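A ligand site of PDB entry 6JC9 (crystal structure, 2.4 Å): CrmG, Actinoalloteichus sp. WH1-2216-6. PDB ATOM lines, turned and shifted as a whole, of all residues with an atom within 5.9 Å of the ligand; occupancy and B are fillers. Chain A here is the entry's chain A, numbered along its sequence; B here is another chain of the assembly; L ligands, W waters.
The side-chain amino group of Lys 344 is covalently linked to a carbon (C5) of the ligand.
The side-chain carboxylate of Asp 315 is in hydrogen-bond range of a nitrogen (N1) of the ligand, 2.9 Å away.
N of Thr 374 of chain B sits at hydrogen-bond distance from O5 of the ligand, 2.9 Å away.
The side-chain hydroxyl (OG1) of Thr 374 of chain B lies within hydrogen-bond range of an oxygen (O5) of the ligand.
The backbone NH of Ala 121 lies within hydrogen-bond range of an oxygen (O4) of the ligand, 3.0 Å away.
NE2 of Gln 318 lies within hydrogen-bond range of O1 of the ligand (3.0 Å).
N of Gly 120 is in hydrogen-bond range of O3 of the ligand, 3.1 Å away.
The side-chain amino group of Lys 344 sits at hydrogen-bond distance from the side-chain hydroxyl of Thr 374 of chain B (2.7 Å).
The backbone carbonyl oxygen of Val 317 is in hydrogen-bond range of the backbone NH of Lys 344.
The side-chain carboxylate (OD2) of Asp 315 lies within hydrogen-bond range of a ring nitrogen (ND1) of His 208, at 2.8 Å.
The side-chain carboxylate (OD2) of Asp 315 sits at hydrogen-bond distance from the side-chain amide nitrogen (ND2) of Asn 124.
OE1 of Glu 282 lies within hydrogen-bond range of N of Phe 207, 2.8 Å away.
The side-chain hydroxyl (OG) of Ser 119 lies within hydrogen-bond range of the side-chain carboxylate (OE2) of Glu 122 of chain B, 2.6 Å away.
The backbone carbonyl oxygen of His 208 lies within hydrogen-bond range of the side-chain amide nitrogen of Asn 124 (3.0 Å).
OG of Ser 373 of chain B sits at hydrogen-bond distance from ND2 of Asn 118 of chain B (3.0 Å).
The backbone carbonyl oxygen (O) of Phe 207 lies close to a nitrogen (N1) of the ligand, 3.3 Å away.
Residues that only touch the ligand: Ser 119 (3.6 Å), Asn 124 (3.98 Å), His 208 (3.6 Å), Gly 209 (3.8 Å), Glu 282 (3.3 Å), Val 317 (3.6 Å) and Ser 373 of chain B (3.7 Å).
Hydrophobic or aromatic side chains that line the ligand: Ala 121, Phe 207 and Val 317.
The nearest printed residue that does not touch the ligand is Phe 375 of chain B (4.1 Å).
Water W2 lies within hydrogen-bond range of OE2 of Glu 122 of chain B, OG of Ser 373 of chain B, O4 of the ligand and OG of Ser 119.
Water W3 lies within hydrogen-bond range of an oxygen (O4) of the ligand (3.0 Å) and the backbone NH of Lys 210 (3.0 Å).
Water W4 bridges O of Val 284 and OE2 of Glu 282.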
ATOM      1  N   PHE A  55      11.977 -10.467 -30.699  1.00  0.00           N
ATOM      2  CA  PHE A  55      12.460  -9.114 -30.357  1.00  0.00           C
ATOM      3  C   PHE A  55      13.981  -9.042 -30.521  1.00  0.00           C
ATOM      4  O   PHE A  55      14.640  -8.441 -29.662  1.00  0.00           O
ATOM      5  CB  PHE A  55      12.025  -8.751 -28.936  1.00  0.00           C
ATOM      6  CG  PHE A  55      10.537  -8.715 -28.719  1.00  0.00           C
ATOM      7  CD1 PHE A  55       9.734  -7.868 -29.460  1.00  0.00           C
ATOM      8  CD2 PHE A  55       9.930  -9.549 -27.798  1.00  0.00           C
ATOM      9  CE1 PHE A  55       8.348  -7.866 -29.291  1.00  0.00           C
ATOM     10  CE2 PHE A  55       8.552  -9.542 -27.619  1.00  0.00           C
ATOM     11  CZ  PHE A  55       7.763  -8.697 -28.369  1.00  0.00           C
ATOM     12  N   ASN A 118      19.480 -16.718 -16.579  1.00  0.00           N
ATOM     13  CA  ASN A 118      18.428 -17.428 -17.347  1.00  0.00           C
ATOM     14  C   ASN A 118      17.615 -16.446 -18.207  1.00  0.00           C
ATOM     15  O   ASN A 118      16.798 -16.922 -19.024  1.00  0.00           O
ATOM     16  CB  ASN A 118      17.550 -18.237 -16.400  1.00  0.00           C
ATOM     17  CG  ASN A 118      18.393 -19.146 -15.525  1.00  0.00           C
ATOM     18  OD1 ASN A 118      19.064 -20.035 -16.037  1.00  0.00           O
ATOM     19  ND2 ASN A 118      18.406 -18.885 -14.220  1.00  0.00           N
ATOM     20  N   SER A 119      17.796 -15.152 -17.992  1.00  0.00           N
ATOM     21  CA  SER A 119      17.072 -14.104 -18.743  1.00  0.00           C
ATOM     22  C   SER A 119      17.870 -12.802 -18.675  1.00  0.00           C
ATOM     23  O   SER A 119      18.768 -12.719 -17.801  1.00  0.00           O
ATOM     24  CB  SER A 119      15.688 -13.915 -18.196  1.00  0.00           C
ATOM     25  OG  SER A 119      15.722 -13.378 -16.908  1.00  0.00           O
ATOM     26  N   GLY A 120      17.551 -11.861 -19.575  1.00  0.00           N
ATOM     27  CA  GLY A 120      18.115 -10.496 -19.576  1.00  0.00           C
ATOM     28  C   GLY A 120      17.847  -9.797 -18.253  1.00  0.00           C
ATOM     29  O   GLY A 120      18.791  -9.176 -17.692  1.00  0.00           O
ATOM     30  N   ALA A 121      16.628  -9.908 -17.749  1.00  0.00           N
ATOM     31  CA  ALA A 121      16.262  -9.326 -16.435  1.00  0.00           C
ATOM     32  C   ALA A 121      17.196  -9.882 -15.361  1.00  0.00           C
ATOM     33  O   ALA A 121      17.745  -9.077 -14.583  1.00  0.00           O
ATOM     34  CB  ALA A 121      14.791  -9.548 -16.096  1.00  0.00           C
ATOM     35  N   GLU A 122      17.397 -11.208 -15.318  1.00  0.00           N
ATOM     36  CA  GLU A 122      18.263 -11.821 -14.268  1.00  0.00           C
ATOM     37  C   GLU A 122      19.691 -11.277 -14.370  1.00  0.00           C
ATOM     38  O   GLU A 122      20.301 -11.032 -13.309  1.00  0.00           O
ATOM     39  CB  GLU A 122      18.290 -13.354 -14.361  1.00  0.00           C
ATOM     40  CG  GLU A 122      16.973 -14.013 -13.977  1.00  0.00           C
ATOM     41  CD  GLU A 122      17.062 -15.509 -13.649  1.00  0.00           C
ATOM     42  OE1 GLU A 122      18.029 -16.193 -14.106  1.00  0.00           O
ATOM     43  OE2 GLU A 122      16.163 -15.977 -12.930  1.00  0.00           O
ATOM     44  N   ASN A 124      20.689  -8.300 -15.701  1.00  0.00           N
ATOM     45  CA  ASN A 124      20.585  -6.903 -15.204  1.00  0.00           C
ATOM     46  C   ASN A 124      20.492  -6.907 -13.673  1.00  0.00           C
ATOM     47  O   ASN A 124      21.104  -6.033 -13.065  1.00  0.00           O
ATOM     48  CB  ASN A 124      19.444  -6.154 -15.900  1.00  0.00           C
ATOM     49  CG  ASN A 124      19.812  -5.760 -17.312  1.00  0.00           C
ATOM     50  OD1 ASN A 124      20.989  -5.810 -17.663  1.00  0.00           O
ATOM     51  ND2 ASN A 124      18.840  -5.318 -18.089  1.00  0.00           N
ATOM     52  N   PHE A 207      14.341   0.319 -21.235  1.00  0.00           N
ATOM     53  CA  PHE A 207      13.758  -1.005 -20.954  1.00  0.00           C
ATOM     54  C   PHE A 207      14.863  -1.930 -20.445  1.00  0.00           C
ATOM     55  O   PHE A 207      15.782  -2.208 -21.269  1.00  0.00           O
ATOM     56  CB  PHE A 207      13.069  -1.563 -22.195  1.00  0.00           C
ATOM     57  CG  PHE A 207      12.325  -2.819 -21.870  1.00  0.00           C
ATOM     58  CD1 PHE A 207      11.022  -2.767 -21.426  1.00  0.00           C
ATOM     59  CD2 PHE A 207      12.979  -4.047 -21.908  1.00  0.00           C
ATOM     60  CE1 PHE A 207      10.361  -3.940 -21.072  1.00  0.00           C
ATOM     61  CE2 PHE A 207      12.316  -5.205 -21.541  1.00  0.00           C
ATOM     62  CZ  PHE A 207      11.018  -5.154 -21.110  1.00  0.00           C
ATOM     63  N   HIS A 208      14.796  -2.396 -19.181  1.00  0.00           N
ATOM     64  CA  HIS A 208      15.850  -3.228 -18.530  1.00  0.00           C
ATOM     65  C   HIS A 208      15.249  -4.518 -17.930  1.00  0.00           C
ATOM     66  O   HIS A 208      15.988  -5.265 -17.222  1.00  0.00           O
ATOM     67  CB  HIS A 208      16.625  -2.402 -17.492  1.00  0.00           C
ATOM     68  CG  HIS A 208      17.376  -1.257 -18.099  1.00  0.00           C
ATOM     69  ND1 HIS A 208      18.308  -1.446 -19.122  1.00  0.00           N
ATOM     70  CD2 HIS A 208      17.351   0.078 -17.848  1.00  0.00           C
ATOM     71  CE1 HIS A 208      18.802  -0.261 -19.492  1.00  0.00           C
ATOM     72  NE2 HIS A 208      18.244   0.694 -18.716  1.00  0.00           N
ATOM     73  N   GLY A 209      13.975  -4.811 -18.225  1.00  0.00           N
ATOM     74  CA  GLY A 209      13.278  -6.015 -17.723  1.00  0.00           C
ATOM     75  C   GLY A 209      12.105  -5.688 -16.823  1.00  0.00           C
ATOM     76  O   GLY A 209      11.806  -4.456 -16.601  1.00  0.00           O
ATOM     77  N   LYS A 210      11.417  -6.735 -16.342  1.00  0.00           N
ATOM     78  CA  LYS A 210      10.076  -6.564 -15.722  1.00  0.00           C
ATOM     79  C   LYS A 210       9.946  -7.378 -14.431  1.00  0.00           C
ATOM     80  O   LYS A 210       8.805  -7.554 -13.961  1.00  0.00           O
ATOM     81  CB  LYS A 210       9.000  -6.889 -16.768  1.00  0.00           C
ATOM     82  CG  LYS A 210       9.180  -6.170 -18.094  1.00  0.00           C
ATOM     83  CD  LYS A 210       8.133  -6.480 -19.122  1.00  0.00           C
ATOM     84  CE  LYS A 210       6.797  -5.819 -18.875  1.00  0.00           C
ATOM     85  NZ  LYS A 210       5.877  -6.087 -19.999  1.00  0.00           N
ATOM     86  N   GLU A 282      21.133   1.400 -22.569  1.00  0.00           N
ATOM     87  CA  GLU A 282      21.051   0.561 -23.789  1.00  0.00           C
ATOM     88  C   GLU A 282      21.761   1.284 -24.929  1.00  0.00           C
ATOM     89  O   GLU A 282      21.377   2.393 -25.277  1.00  0.00           O
ATOM     90  CB  GLU A 282      19.601   0.313 -24.197  1.00  0.00           C
ATOM     91  CG  GLU A 282      18.708  -0.279 -23.133  1.00  0.00           C
ATOM     92  CD  GLU A 282      17.234  -0.162 -23.512  1.00  0.00           C
ATOM     93  OE1 GLU A 282      16.531   0.653 -22.879  1.00  0.00           O
ATOM     94  OE2 GLU A 282      16.800  -0.863 -24.457  1.00  0.00           O
ATOM     95  N   VAL A 284      21.258   0.935 -28.027  1.00  0.00           N
ATOM     96  CA  VAL A 284      20.093   1.231 -28.919  1.00  0.00           C
ATOM     97  C   VAL A 284      18.848   1.024 -28.061  1.00  0.00           C
ATOM     98  O   VAL A 284      18.713  -0.078 -27.504  1.00  0.00           O
ATOM     99  CB  VAL A 284      20.085   0.370 -30.193  1.00  0.00           C
ATOM    100  CG1 VAL A 284      19.033   0.862 -31.204  1.00  0.00           C
ATOM    101  CG2 VAL A 284      21.464   0.322 -30.866  1.00  0.00           C
ATOM    102  N   GLY A 286      15.402   0.294 -27.120  1.00  0.00           N
ATOM    103  CA  GLY A 286      14.192  -0.458 -27.483  1.00  0.00           C
ATOM    104  C   GLY A 286      12.890   0.252 -27.133  1.00  0.00           C
ATOM    105  O   GLY A 286      12.065   0.487 -28.074  1.00  0.00           O
ATOM    106  N   ASP A 315      23.485  -2.394 -21.019  1.00  0.00           N
ATOM    107  CA  ASP A 315      22.474  -3.455 -21.273  1.00  0.00           C
ATOM    108  C   ASP A 315      22.501  -3.763 -22.774  1.00  0.00           C
ATOM    109  O   ASP A 315      21.967  -2.962 -23.547  1.00  0.00           O
ATOM    110  CB  ASP A 315      21.093  -3.029 -20.747  1.00  0.00           C
ATOM    111  CG  ASP A 315      19.979  -4.048 -20.947  1.00  0.00           C
ATOM    112  OD1 ASP A 315      20.159  -4.984 -21.787  1.00  0.00           O
ATOM    113  OD2 ASP A 315      18.913  -3.897 -20.282  1.00  0.00           O
ATOM    114  N   VAL A 317      21.424  -6.771 -23.867  1.00  0.00           N
ATOM    115  CA  VAL A 317      20.478  -7.913 -23.975  1.00  0.00           C
ATOM    116  C   VAL A 317      19.893  -7.983 -25.403  1.00  0.00           C
ATOM    117  O   VAL A 317      19.797  -9.101 -25.915  1.00  0.00           O
ATOM    118  CB  VAL A 317      19.391  -7.808 -22.918  1.00  0.00           C
ATOM    119  CG1 VAL A 317      18.196  -8.671 -23.291  1.00  0.00           C
ATOM    120  CG2 VAL A 317      19.968  -8.161 -21.551  1.00  0.00           C
ATOM    121  N   GLN A 318      19.602  -6.837 -26.030  1.00  0.00           N
ATOM    122  CA  GLN A 318      18.982  -6.765 -27.381  1.00  0.00           C
ATOM    123  C   GLN A 318      20.026  -6.406 -28.446  1.00  0.00           C
ATOM    124  O   GLN A 318      19.946  -7.017 -29.558  1.00  0.00           O
ATOM    125  CB  GLN A 318      17.845  -5.750 -27.351  1.00  0.00           C
ATOM    126  CG  GLN A 318      16.742  -6.056 -28.348  1.00  0.00           C
ATOM    127  CD  GLN A 318      15.717  -4.965 -28.544  1.00  0.00           C
ATOM    128  OE1 GLN A 318      15.289  -4.727 -29.667  1.00  0.00           O
ATOM    129  NE2 GLN A 318      15.303  -4.318 -27.476  1.00  0.00           N
ATOM    130  N   ALA A 343      21.930 -11.454 -23.520  1.00  0.00           N
ATOM    131  CA  ALA A 343      20.936 -12.547 -23.437  1.00  0.00           C
ATOM    132  C   ALA A 343      20.453 -12.933 -24.842  1.00  0.00           C
ATOM    133  O   ALA A 343      21.039 -13.812 -25.412  1.00  0.00           O
ATOM    134  CB  ALA A 343      19.831 -12.118 -22.515  1.00  0.00           C
ATOM    135  N   LYS A 344      19.476 -12.228 -25.400  1.00  0.00           N
ATOM    136  CA  LYS A 344      18.551 -12.706 -26.459  1.00  0.00           C
ATOM    137  C   LYS A 344      19.254 -13.745 -27.385  1.00  0.00           C
ATOM    138  O   LYS A 344      18.976 -14.969 -27.230  1.00  0.00           O
ATOM    139  CB  LYS A 344      17.846 -11.491 -27.091  1.00  0.00           C
ATOM    140  CG  LYS A 344      16.915 -10.737 -26.133  1.00  0.00           C
ATOM    141  CD  LYS A 344      15.748  -9.920 -26.760  1.00  0.00           C
ATOM    142  CE  LYS A 344      15.239  -8.685 -26.013  1.00  0.00           C
ATOM    143  NZ  LYS A 344      14.688  -8.832 -24.622  1.00  0.00           N
ATOM    144  N   ASN B 118      10.959 -18.134 -16.421  1.00  0.00           N
ATOM    145  CA  ASN B 118      12.232 -18.786 -16.855  1.00  0.00           C
ATOM    146  C   ASN B 118      12.980 -19.394 -15.654  1.00  0.00           C
ATOM    147  O   ASN B 118      13.972 -20.102 -15.870  1.00  0.00           O
ATOM    148  CB  ASN B 118      13.069 -17.764 -17.625  1.00  0.00           C
ATOM    149  CG  ASN B 118      12.270 -17.140 -18.748  1.00  0.00           C
ATOM    150  OD1 ASN B 118      11.863 -17.863 -19.664  1.00  0.00           O
ATOM    151  ND2 ASN B 118      11.993 -15.845 -18.651  1.00  0.00           N
ATOM    152  N   GLU B 122      11.819 -16.059 -10.820  1.00  0.00           N
ATOM    153  CA  GLU B 122      10.922 -15.234 -11.690  1.00  0.00           C
ATOM    154  C   GLU B 122       9.451 -15.556 -11.375  1.00  0.00           C
ATOM    155  O   GLU B 122       8.634 -14.606 -11.378  1.00  0.00           O
ATOM    156  CB  GLU B 122      11.184 -15.445 -13.176  1.00  0.00           C
ATOM    157  CG  GLU B 122      12.506 -14.886 -13.674  1.00  0.00           C
ATOM    158  CD  GLU B 122      12.641 -14.753 -15.188  1.00  0.00           C
ATOM    159  OE1 GLU B 122      11.895 -15.425 -15.955  1.00  0.00           O
ATOM    160  OE2 GLU B 122      13.512 -13.975 -15.607  1.00  0.00           O
ATOM    161  N   SER B 372       5.370  -9.447 -18.948  1.00  0.00           N
ATOM    162  CA  SER B 372       5.888 -10.302 -20.052  1.00  0.00           C
ATOM    163  C   SER B 372       7.390 -10.573 -19.843  1.00  0.00           C
ATOM    164  O   SER B 372       7.952 -10.034 -18.889  1.00  0.00           O
ATOM    165  CB  SER B 372       5.616  -9.679 -21.404  1.00  0.00           C
ATOM    166  OG  SER B 372       6.259  -8.415 -21.488  1.00  0.00           O
ATOM    167  N   SER B 373       7.987 -11.361 -20.735  1.00  0.00           N
ATOM    168  CA  SER B 373       9.410 -11.770 -20.748  1.00  0.00           C
ATOM    169  C   SER B 373       9.710 -12.337 -22.136  1.00  0.00           C
ATOM    170  O   SER B 373       8.857 -13.079 -22.606  1.00  0.00           O
ATOM    171  CB  SER B 373       9.655 -12.815 -19.673  1.00  0.00           C
ATOM    172  OG  SER B 373      11.030 -13.165 -19.594  1.00  0.00           O
ATOM    173  N   THR B 374      10.854 -12.043 -22.735  1.00  0.00           N
ATOM    174  CA  THR B 374      11.260 -12.539 -24.077  1.00  0.00           C
ATOM    175  C   THR B 374      11.095 -14.070 -24.132  1.00  0.00           C
ATOM    176  O   THR B 374      10.426 -14.566 -25.048  1.00  0.00           O
ATOM    177  CB  THR B 374      12.677 -12.089 -24.436  1.00  0.00           C
ATOM    178  OG1 THR B 374      12.676 -10.653 -24.427  1.00  0.00           O
ATOM    179  CG2 THR B 374      13.157 -12.599 -25.777  1.00  0.00           C
ATOM    180  N   PHE B 375      11.702 -14.773 -23.198  1.00  0.00           N
ATOM    181  CA  PHE B 375      11.885 -16.245 -23.237  1.00  0.00           C
ATOM    182  C   PHE B 375      10.672 -16.965 -22.632  1.00  0.00           C
ATOM    183  O   PHE B 375      10.561 -18.172 -22.839  1.00  0.00           O
ATOM    184  CB  PHE B 375      13.145 -16.666 -22.475  1.00  0.00           C
ATOM    185  CG  PHE B 375      14.481 -16.260 -23.056  1.00  0.00           C
ATOM    186  CD1 PHE B 375      14.690 -16.239 -24.433  1.00  0.00           C
ATOM    187  CD2 PHE B 375      15.560 -15.982 -22.227  1.00  0.00           C
ATOM    188  CE1 PHE B 375      15.933 -15.909 -24.964  1.00  0.00           C
ATOM    189  CE2 PHE B 375      16.800 -15.658 -22.751  1.00  0.00           C
ATOM    190  CZ  PHE B 375      16.988 -15.619 -24.123  1.00  0.00           C
HETATM  191  N1  LIG L   1      16.803  -5.292 -21.608  1.00  0.00           N
HETATM  192  C1  LIG L   1      16.494  -5.140 -22.899  1.00  0.00           C
HETATM  193  C2  LIG L   1      17.098  -3.992 -23.627  1.00  0.00           C
HETATM  194  C3  LIG L   1      15.610  -6.024 -23.549  1.00  0.00           C
HETATM  195  O1  LIG L   1      15.294  -5.805 -24.839  1.00  0.00           O
HETATM  196  C4  LIG L   1      15.037  -7.105 -22.858  1.00  0.00           C
HETATM  197  C5  LIG L   1      14.190  -8.016 -23.637  1.00  0.00           C
HETATM  198  C6  LIG L   1      15.382  -7.231 -21.485  1.00  0.00           C
HETATM  199  C7  LIG L   1      16.246  -6.319 -20.930  1.00  0.00           C
HETATM  200  C8  LIG L   1      14.850  -8.324 -20.609  1.00  0.00           C
HETATM  201  O2  LIG L   1      15.228  -9.631 -21.108  1.00  0.00           O
HETATM  202  P1  LIG L   1      14.245 -10.855 -20.698  1.00  0.00           P
HETATM  203  O3  LIG L   1      14.973 -12.080 -21.250  1.00  0.00           O
HETATM  204  O4  LIG L   1      14.163 -10.776 -19.153  1.00  0.00           O
HETATM  205  O5  LIG L   1      12.939 -10.564 -21.387  1.00  0.00           O
HETATM  206  O   HOH W   1      13.222 -13.840 -20.937  1.00  0.00           O
HETATM  207  O   HOH W   2      12.606 -12.500 -17.523  1.00  0.00           O
HETATM  208  O   HOH W   3      11.901  -9.158 -18.066  1.00  0.00           O
HETATM  209  O   HOH W   4      18.098  -2.204 -26.421  1.00  0.00           O
HETATM  210  O   HOH W   5      11.049  -8.562 -20.548  1.00  0.00           O
